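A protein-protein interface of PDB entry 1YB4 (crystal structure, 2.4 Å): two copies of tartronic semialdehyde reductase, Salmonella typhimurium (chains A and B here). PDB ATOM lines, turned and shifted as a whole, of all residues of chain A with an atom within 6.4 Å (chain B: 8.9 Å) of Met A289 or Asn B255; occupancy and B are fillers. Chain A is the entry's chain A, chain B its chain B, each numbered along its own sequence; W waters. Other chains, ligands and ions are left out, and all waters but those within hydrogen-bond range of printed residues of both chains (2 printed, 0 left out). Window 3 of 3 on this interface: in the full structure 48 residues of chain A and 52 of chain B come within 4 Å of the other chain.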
ATOM      1  N   GLU A 184     -27.204  24.160 -16.295  1.00  0.00           N
ATOM      2  CA  GLU A 184     -26.661  23.022 -15.574  1.00  0.00           C
ATOM      3  C   GLU A 184     -26.352  23.420 -14.135  1.00  0.00           C
ATOM      4  O   GLU A 184     -26.543  22.633 -13.201  1.00  0.00           O
ATOM      5  CB  GLU A 184     -25.409  22.510 -16.285  1.00  0.00           C
ATOM      6  CG  GLU A 184     -25.028  21.067 -15.962  1.00  0.00           C
ATOM      7  CD  GLU A 184     -24.215  20.934 -14.689  1.00  0.00           C
ATOM      8  OE1 GLU A 184     -23.645  21.951 -14.230  1.00  0.00           O
ATOM      9  OE2 GLU A 184     -24.127  19.802 -14.161  1.00  0.00           O
ATOM     10  N   GLU A 188     -27.685  21.576 -10.646  1.00  0.00           N
ATOM     11  CA  GLU A 188     -26.846  20.970  -9.619  1.00  0.00           C
ATOM     12  C   GLU A 188     -27.139  21.537  -8.234  1.00  0.00           C
ATOM     13  O   GLU A 188     -27.145  20.808  -7.246  1.00  0.00           O
ATOM     14  CB  GLU A 188     -25.362  21.179  -9.956  1.00  0.00           C
ATOM     15  CG  GLU A 188     -24.805  20.179 -10.948  1.00  0.00           C
ATOM     16  CD  GLU A 188     -23.285  20.249 -11.098  1.00  0.00           C
ATOM     17  OE1 GLU A 188     -22.572  20.506 -10.095  1.00  0.00           O
ATOM     18  OE2 GLU A 188     -22.796  20.018 -12.226  1.00  0.00           O
ATOM     19  N   LEU A 265     -24.068  15.523 -20.750  1.00  0.00           N
ATOM     20  CA  LEU A 265     -25.267  15.454 -19.919  1.00  0.00           C
ATOM     21  C   LEU A 265     -26.512  15.504 -20.833  1.00  0.00           C
ATOM     22  O   LEU A 265     -27.523  14.846 -20.566  1.00  0.00           O
ATOM     23  CB  LEU A 265     -25.279  16.605 -18.906  1.00  0.00           C
ATOM     24  CG  LEU A 265     -24.210  16.605 -17.796  1.00  0.00           C
ATOM     25  CD1 LEU A 265     -24.317  17.884 -16.991  1.00  0.00           C
ATOM     26  CD2 LEU A 265     -24.388  15.407 -16.883  1.00  0.00           C
ATOM     27  N   THR A 268     -27.308  12.256 -21.986  1.00  0.00           N
ATOM     28  CA  THR A 268     -28.055  11.468 -21.015  1.00  0.00           C
ATOM     29  C   THR A 268     -29.540  11.820 -21.143  1.00  0.00           C
ATOM     30  O   THR A 268     -30.391  10.946 -21.050  1.00  0.00           O
ATOM     31  CB  THR A 268     -27.517  11.716 -19.570  1.00  0.00           C
ATOM     32  OG1 THR A 268     -26.231  11.095 -19.440  1.00  0.00           O
ATOM     33  CG2 THR A 268     -28.445  11.122 -18.507  1.00  0.00           C
ATOM     34  N   MET A 282     -32.788  19.777 -18.654  1.00  0.00           N
ATOM     35  CA  MET A 282     -31.440  19.391 -18.274  1.00  0.00           C
ATOM     36  C   MET A 282     -31.439  18.796 -16.879  1.00  0.00           C
ATOM     37  O   MET A 282     -30.768  17.802 -16.624  1.00  0.00           O
ATOM     38  CB  MET A 282     -30.536  20.632 -18.292  1.00  0.00           C
ATOM     39  CG  MET A 282     -29.214  20.507 -17.548  1.00  0.00           C
ATOM     40  SD  MET A 282     -27.961  19.361 -18.455  1.00  0.00           S
ATOM     41  CE  MET A 282     -28.001  17.886 -17.268  1.00  0.00           C
ATOM     42  N   GLN A 284     -33.243  16.935 -15.344  1.00  0.00           N
ATOM     43  CA  GLN A 284     -33.549  15.514 -15.244  1.00  0.00           C
ATOM     44  C   GLN A 284     -32.291  14.648 -15.255  1.00  0.00           C
ATOM     45  O   GLN A 284     -32.266  13.580 -14.647  1.00  0.00           O
ATOM     46  CB  GLN A 284     -34.487  15.094 -16.382  1.00  0.00           C
ATOM     47  CG  GLN A 284     -35.839  15.788 -16.330  1.00  0.00           C
ATOM     48  CD  GLN A 284     -36.850  15.172 -17.275  1.00  0.00           C
ATOM     49  OE1 GLN A 284     -36.714  15.259 -18.496  1.00  0.00           O
ATOM     50  NE2 GLN A 284     -37.868  14.534 -16.710  1.00  0.00           N
ATOM     51  N   ALA A 285     -31.248  15.111 -15.939  1.00  0.00           N
ATOM     52  CA  ALA A 285     -30.014  14.344 -16.010  1.00  0.00           C
ATOM     53  C   ALA A 285     -29.390  14.220 -14.642  1.00  0.00           C
ATOM     54  O   ALA A 285     -28.933  13.149 -14.262  1.00  0.00           O
ATOM     55  CB  ALA A 285     -29.048  14.984 -16.966  1.00  0.00           C
ATOM     56  N   LEU A 286     -29.369  15.316 -13.891  1.00  0.00           N
ATOM     57  CA  LEU A 286     -28.797  15.254 -12.557  1.00  0.00           C
ATOM     58  C   LEU A 286     -29.731  14.547 -11.577  1.00  0.00           C
ATOM     59  O   LEU A 286     -29.277  13.936 -10.606  1.00  0.00           O
ATOM     60  CB  LEU A 286     -28.434  16.652 -12.070  1.00  0.00           C
ATOM     61  CG  LEU A 286     -27.271  17.137 -12.934  1.00  0.00           C
ATOM     62  CD1 LEU A 286     -27.802  17.840 -14.148  1.00  0.00           C
ATOM     63  CD2 LEU A 286     -26.411  18.047 -12.156  1.00  0.00           C
ATOM     64  N   GLU A 287     -31.037  14.618 -11.826  1.00  0.00           N
ATOM     65  CA  GLU A 287     -31.979  13.929 -10.947  1.00  0.00           C
ATOM     66  C   GLU A 287     -31.700  12.438 -11.109  1.00  0.00           C
ATOM     67  O   GLU A 287     -31.648  11.703 -10.134  1.00  0.00           O
ATOM     68  CB  GLU A 287     -33.429  14.248 -11.324  1.00  0.00           C
ATOM     69  CG  GLU A 287     -33.838  15.677 -11.004  1.00  0.00           C
ATOM     70  CD  GLU A 287     -35.220  16.021 -11.529  1.00  0.00           C
ATOM     71  OE1 GLU A 287     -35.540  15.594 -12.656  1.00  0.00           O
ATOM     72  OE2 GLU A 287     -35.978  16.726 -10.833  1.00  0.00           O
ATOM     73  N   LEU A 288     -31.490  12.004 -12.348  1.00  0.00           N
ATOM     74  CA  LEU A 288     -31.209  10.597 -12.640  1.00  0.00           C
ATOM     75  C   LEU A 288     -29.920  10.142 -11.946  1.00  0.00           C
ATOM     76  O   LEU A 288     -29.872   9.074 -11.318  1.00  0.00           O
ATOM     77  CB  LEU A 288     -31.071  10.406 -14.155  1.00  0.00           C
ATOM     78  CG  LEU A 288     -30.800   8.994 -14.680  1.00  0.00           C
ATOM     79  CD1 LEU A 288     -31.939   8.089 -14.292  1.00  0.00           C
ATOM     80  CD2 LEU A 288     -30.654   9.013 -16.198  1.00  0.00           C
ATOM     81  N   MET A 289     -28.886  10.975 -12.062  1.00  0.00           N
ATOM     82  CA  MET A 289     -27.582  10.686 -11.493  1.00  0.00           C
ATOM     83  C   MET A 289     -27.531  10.744  -9.969  1.00  0.00           C
ATOM     84  O   MET A 289     -26.546  10.322  -9.361  1.00  0.00           O
ATOM     85  CB  MET A 289     -26.550  11.632 -12.118  1.00  0.00           C
ATOM     86  CG  MET A 289     -26.330  11.365 -13.617  1.00  0.00           C
ATOM     87  SD  MET A 289     -25.780  12.887 -14.702  1.00  0.00           S
ATOM     88  CE  MET A 289     -23.875  12.825 -14.339  1.00  0.00           C
ATOM     89  N   ALA A 290     -28.595  11.246  -9.355  1.00  0.00           N
ATOM     90  CA  ALA A 290     -28.660  11.351  -7.910  1.00  0.00           C
ATOM     91  C   ALA A 290     -29.816  10.519  -7.379  1.00  0.00           C
ATOM     92  O   ALA A 290     -29.932  10.302  -6.168  1.00  0.00           O
ATOM     93  CB  ALA A 290     -28.843  12.804  -7.508  1.00  0.00           C
ATOM     94  N   ASN A 291     -30.657  10.031  -8.286  1.00  0.00           N
ATOM     95  CA  ASN A 291     -31.832   9.248  -7.906  1.00  0.00           C
ATOM     96  C   ASN A 291     -32.667  10.097  -6.940  1.00  0.00           C
ATOM     97  O   ASN A 291     -33.018   9.660  -5.847  1.00  0.00           O
ATOM     98  CB  ASN A 291     -31.422   7.936  -7.225  1.00  0.00           C
ATOM     99  CG  ASN A 291     -32.558   6.908  -7.207  1.00  0.00           C
ATOM    100  OD1 ASN A 291     -33.617   7.120  -7.819  1.00  0.00           O
ATOM    101  ND2 ASN A 291     -32.339   5.788  -6.518  1.00  0.00           N
ATOM    102  N   HIS A 292     -32.966  11.323  -7.356  1.00  0.00           N
ATOM    103  CA  HIS A 292     -33.751  12.240  -6.549  1.00  0.00           C
ATOM    104  C   HIS A 292     -34.280  13.382  -7.432  1.00  0.00           C
ATOM    105  O   HIS A 292     -33.503  14.181  -7.954  1.00  0.00           O
ATOM    106  CB  HIS A 292     -32.873  12.779  -5.426  1.00  0.00           C
ATOM    107  CG  HIS A 292     -33.615  13.572  -4.408  1.00  0.00           C
ATOM    108  ND1 HIS A 292     -34.143  14.815  -4.678  1.00  0.00           N
ATOM    109  CD2 HIS A 292     -33.930  13.298  -3.123  1.00  0.00           C
ATOM    110  CE1 HIS A 292     -34.751  15.274  -3.601  1.00  0.00           C
ATOM    111  NE2 HIS A 292     -34.638  14.372  -2.643  1.00  0.00           N
ATOM    112  N   ALA B 245     -19.473  21.830  -0.308  1.00  0.00           N
ATOM    113  CA  ALA B 245     -20.407  21.335  -1.310  1.00  0.00           C
ATOM    114  C   ALA B 245     -20.133  19.865  -1.637  1.00  0.00           C
ATOM    115  O   ALA B 245     -20.988  19.000  -1.490  1.00  0.00           O
ATOM    116  CB  ALA B 245     -20.276  22.161  -2.576  1.00  0.00           C
ATOM    117  N   LEU B 246     -18.927  19.591  -2.095  1.00  0.00           N
ATOM    118  CA  LEU B 246     -18.576  18.236  -2.462  1.00  0.00           C
ATOM    119  C   LEU B 246     -18.706  17.211  -1.332  1.00  0.00           C
ATOM    120  O   LEU B 246     -19.192  16.095  -1.559  1.00  0.00           O
ATOM    121  CB  LEU B 246     -17.168  18.238  -3.059  1.00  0.00           C
ATOM    122  CG  LEU B 246     -17.193  19.115  -4.316  1.00  0.00           C
ATOM    123  CD1 LEU B 246     -15.800  19.356  -4.866  1.00  0.00           C
ATOM    124  CD2 LEU B 246     -18.070  18.434  -5.342  1.00  0.00           C
ATOM    125  N   SER B 248     -20.760  17.300   1.063  1.00  0.00           N
ATOM    126  CA  SER B 248     -22.198  17.081   1.267  1.00  0.00           C
ATOM    127  C   SER B 248     -22.695  16.175   0.165  1.00  0.00           C
ATOM    128  O   SER B 248     -23.487  15.254   0.392  1.00  0.00           O
ATOM    129  CB  SER B 248     -22.960  18.402   1.224  1.00  0.00           C
ATOM    130  OG  SER B 248     -22.487  19.276   2.236  1.00  0.00           O
ATOM    131  N   ALA B 249     -22.217  16.457  -1.041  1.00  0.00           N
ATOM    132  CA  ALA B 249     -22.546  15.664  -2.211  1.00  0.00           C
ATOM    133  C   ALA B 249     -22.164  14.202  -1.918  1.00  0.00           C
ATOM    134  O   ALA B 249     -22.914  13.270  -2.213  1.00  0.00           O
ATOM    135  CB  ALA B 249     -21.764  16.176  -3.413  1.00  0.00           C
ATOM    136  N   LYS B 250     -20.988  14.006  -1.341  1.00  0.00           N
ATOM    137  CA  LYS B 250     -20.563  12.652  -1.034  1.00  0.00           C
ATOM    138  C   LYS B 250     -21.510  12.041  -0.012  1.00  0.00           C
ATOM    139  O   LYS B 250     -21.985  10.921  -0.200  1.00  0.00           O
ATOM    140  CB  LYS B 250     -19.131  12.628  -0.490  1.00  0.00           C
ATOM    141  CG  LYS B 250     -18.573  11.229  -0.298  1.00  0.00           C
ATOM    142  CD  LYS B 250     -17.255  11.256   0.469  1.00  0.00           C
ATOM    143  CE  LYS B 250     -16.916   9.868   1.016  1.00  0.00           C
ATOM    144  NZ  LYS B 250     -15.912   9.918   2.121  1.00  0.00           N
ATOM    145  N   LEU B 252     -24.651  12.878   0.754  1.00  0.00           N
ATOM    146  CA  LEU B 252     -25.997  12.685   0.219  1.00  0.00           C
ATOM    147  C   LEU B 252     -26.049  11.857  -1.078  1.00  0.00           C
ATOM    148  O   LEU B 252     -27.133  11.611  -1.606  1.00  0.00           O
ATOM    149  CB  LEU B 252     -26.663  14.044  -0.037  1.00  0.00           C
ATOM    150  CG  LEU B 252     -26.786  14.929   1.197  1.00  0.00           C
ATOM    151  CD1 LEU B 252     -27.598  16.160   0.885  1.00  0.00           C
ATOM    152  CD2 LEU B 252     -27.431  14.128   2.298  1.00  0.00           C
ATOM    153  N   ALA B 253     -24.882  11.433  -1.572  1.00  0.00           N
ATOM    154  CA  ALA B 253     -24.737  10.662  -2.819  1.00  0.00           C
ATOM    155  C   ALA B 253     -25.265  11.487  -3.991  1.00  0.00           C
ATOM    156  O   ALA B 253     -26.241  11.119  -4.642  1.00  0.00           O
ATOM    157  CB  ALA B 253     -25.485   9.310  -2.731  1.00  0.00           C
ATOM    158  N   LEU B 254     -24.623  12.620  -4.245  1.00  0.00           N
ATOM    159  CA  LEU B 254     -25.025  13.499  -5.339  1.00  0.00           C
ATOM    160  C   LEU B 254     -23.896  13.608  -6.341  1.00  0.00           C
ATOM    161  O   LEU B 254     -22.722  13.730  -5.967  1.00  0.00           O
ATOM    162  CB  LEU B 254     -25.340  14.903  -4.821  1.00  0.00           C
ATOM    163  CG  LEU B 254     -26.664  15.130  -4.112  1.00  0.00           C
ATOM    164  CD1 LEU B 254     -26.620  16.421  -3.324  1.00  0.00           C
ATOM    165  CD2 LEU B 254     -27.767  15.195  -5.151  1.00  0.00           C
ATOM    166  N   ASN B 255     -24.256  13.574  -7.616  1.00  0.00           N
ATOM    167  CA  ASN B 255     -23.272  13.697  -8.681  1.00  0.00           C
ATOM    168  C   ASN B 255     -23.294  15.145  -9.180  1.00  0.00           C
ATOM    169  O   ASN B 255     -24.180  15.519  -9.951  1.00  0.00           O
ATOM    170  CB  ASN B 255     -23.624  12.749  -9.831  1.00  0.00           C
ATOM    171  CG  ASN B 255     -22.531  12.663 -10.874  1.00  0.00           C
ATOM    172  OD1 ASN B 255     -21.929  13.668 -11.241  1.00  0.00           O
ATOM    173  ND2 ASN B 255     -22.280  11.463 -11.370  1.00  0.00           N
ATOM    174  N   LEU B 256     -22.339  15.957  -8.728  1.00  0.00           N
ATOM    175  CA  LEU B 256     -22.258  17.358  -9.150  1.00  0.00           C
ATOM    176  C   LEU B 256     -21.010  17.530 -10.024  1.00  0.00           C
ATOM    177  O   LEU B 256     -19.994  18.099  -9.599  1.00  0.00           O
ATOM    178  CB  LEU B 256     -22.189  18.293  -7.932  1.00  0.00           C
ATOM    179  CG  LEU B 256     -23.147  18.011  -6.766  1.00  0.00           C
ATOM    180  CD1 LEU B 256     -23.295  19.278  -5.955  1.00  0.00           C
ATOM    181  CD2 LEU B 256     -24.518  17.580  -7.257  1.00  0.00           C
ATOM    182  N   PRO B 257     -21.093  17.064 -11.283  1.00  0.00           N
ATOM    183  CA  PRO B 257     -19.999  17.126 -12.256  1.00  0.00           C
ATOM    184  C   PRO B 257     -19.315  18.459 -12.454  1.00  0.00           C
ATOM    185  O   PRO B 257     -18.100  18.503 -12.545  1.00  0.00           O
ATOM    186  CB  PRO B 257     -20.642  16.606 -13.535  1.00  0.00           C
ATOM    187  CG  PRO B 257     -22.069  17.018 -13.377  1.00  0.00           C
ATOM    188  CD  PRO B 257     -22.354  16.693 -11.948  1.00  0.00           C
ATOM    189  N   ASN B 258     -20.062  19.551 -12.518  1.00  0.00           N
ATOM    190  CA  ASN B 258     -19.408  20.838 -12.728  1.00  0.00           C
ATOM    191  C   ASN B 258     -18.877  21.518 -11.445  1.00  0.00           C
ATOM    192  O   ASN B 258     -17.980  22.353 -11.502  1.00  0.00           O
ATOM    193  CB  ASN B 258     -20.334  21.747 -13.554  1.00  0.00           C
ATOM    194  CG  ASN B 258     -20.432  21.289 -15.018  1.00  0.00           C
ATOM    195  OD1 ASN B 258     -20.082  20.156 -15.344  1.00  0.00           O
ATOM    196  ND2 ASN B 258     -20.904  22.163 -15.891  1.00  0.00           N
ATOM    197  N   THR B 259     -19.401  21.140 -10.284  1.00  0.00           N
ATOM    198  CA  THR B 259     -18.895  21.692  -9.029  1.00  0.00           C
ATOM    199  C   THR B 259     -17.528  21.018  -8.799  1.00  0.00           C
ATOM    200  O   THR B 259     -16.571  21.655  -8.366  1.00  0.00           O
ATOM    201  CB  THR B 259     -19.799  21.336  -7.826  1.00  0.00           C
ATOM    202  OG1 THR B 259     -21.101  21.903  -7.999  1.00  0.00           O
ATOM    203  CG2 THR B 259     -19.200  21.857  -6.553  1.00  0.00           C
ATOM    204  N   ALA B 260     -17.443  19.721  -9.078  1.00  0.00           N
ATOM    205  CA  ALA B 260     -16.192  18.989  -8.887  1.00  0.00           C
ATOM    206  C   ALA B 260     -15.103  19.579  -9.774  1.00  0.00           C
ATOM    207  O   ALA B 260     -13.976  19.788  -9.328  1.00  0.00           O
ATOM    208  CB  ALA B 260     -16.387  17.515  -9.205  1.00  0.00           C
HETATM  209  O   HOH W   1     -26.463  14.018  -9.113  1.00  0.00           O
HETATM  210  O   HOH W   2     -22.000  24.605 -14.970  1.00  0.00           O
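OE1 of Glu A184 lies within hydrogen-bond range of ND2 of Asn B258, at 3.2 Å. OE2 of Glu A188 is in hydrogen-bond range of N of Asn B258 (2.8 Å). The side-chain hydroxyl (OG1) of Thr B259 sits at hydrogen-bond distance from the side-chain carboxylate (OE1) of Glu A188 (2.9 Å).
O of Ala B249 is in hydrogen-bond range of N of Leu B254 (2.7 Å).
Glu A184 touches Pro B257 (OE2 to CG, 3.5 Å). Leu B256 touches Glu A188. OE2 of Glu A188 touches CG of Pro B257, 3.3 Å away. Met A289 touches Asn B255 (CE to ND2, 3.6 Å). Ala A290 touches Leu B254 (CB to CD2, 3.5 Å).
Met A289 touches one residue of chain B. Asn B255 touches one residue of chain A. Printed residues of chain B within 4 Å of Ala A290: Leu B254 (3.5 Å). Of the printed residues of chain B, Glu A184 touches Pro B257 and Asn B258. Printed residues of chain A within 4 Å of Thr B259: Glu A188 (2.9 Å). Gln A284 touches none of the printed residues of chain B. Ala A285 touches none of the printed residues of chain B. The nearest residue of chain B that does not touch Met A289 is Pro B257 (4.7 Å). The nearest residue of chain A that does not touch Asn B255 is Leu A286 (4.03 Å). The nearest printed residue of chain B that does not touch Glu A188 is Asn B255 (4.8 Å).
Printed residues of chain A that touch a printed residue of chain B: Glu A184, Glu A188, Met A289 and Ala A290. Hydrophobic or aromatic side chains of chain B that line the printed part of chain A: Leu B254, Leu B256 and Pro B257. Among the printed residues, no Asp or Glu carboxylate lies within 4 Å of a Lys or Arg side-chain nitrogen of the other chain.
No position is printed for both chains. Of the 8 pairs that touch across the chains among the printed residues, none has its exchanged pair printed and touching as well.
Water W1 lies within hydrogen-bond range of N of Asn B255 (2.7 Å) and O of Leu A286 (3.2 Å). Water W2 lies within hydrogen-bond range of the side-chain amide nitrogen (ND2) of Asn B258 and the side-chain carboxylate (OE1) of Glu A184.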
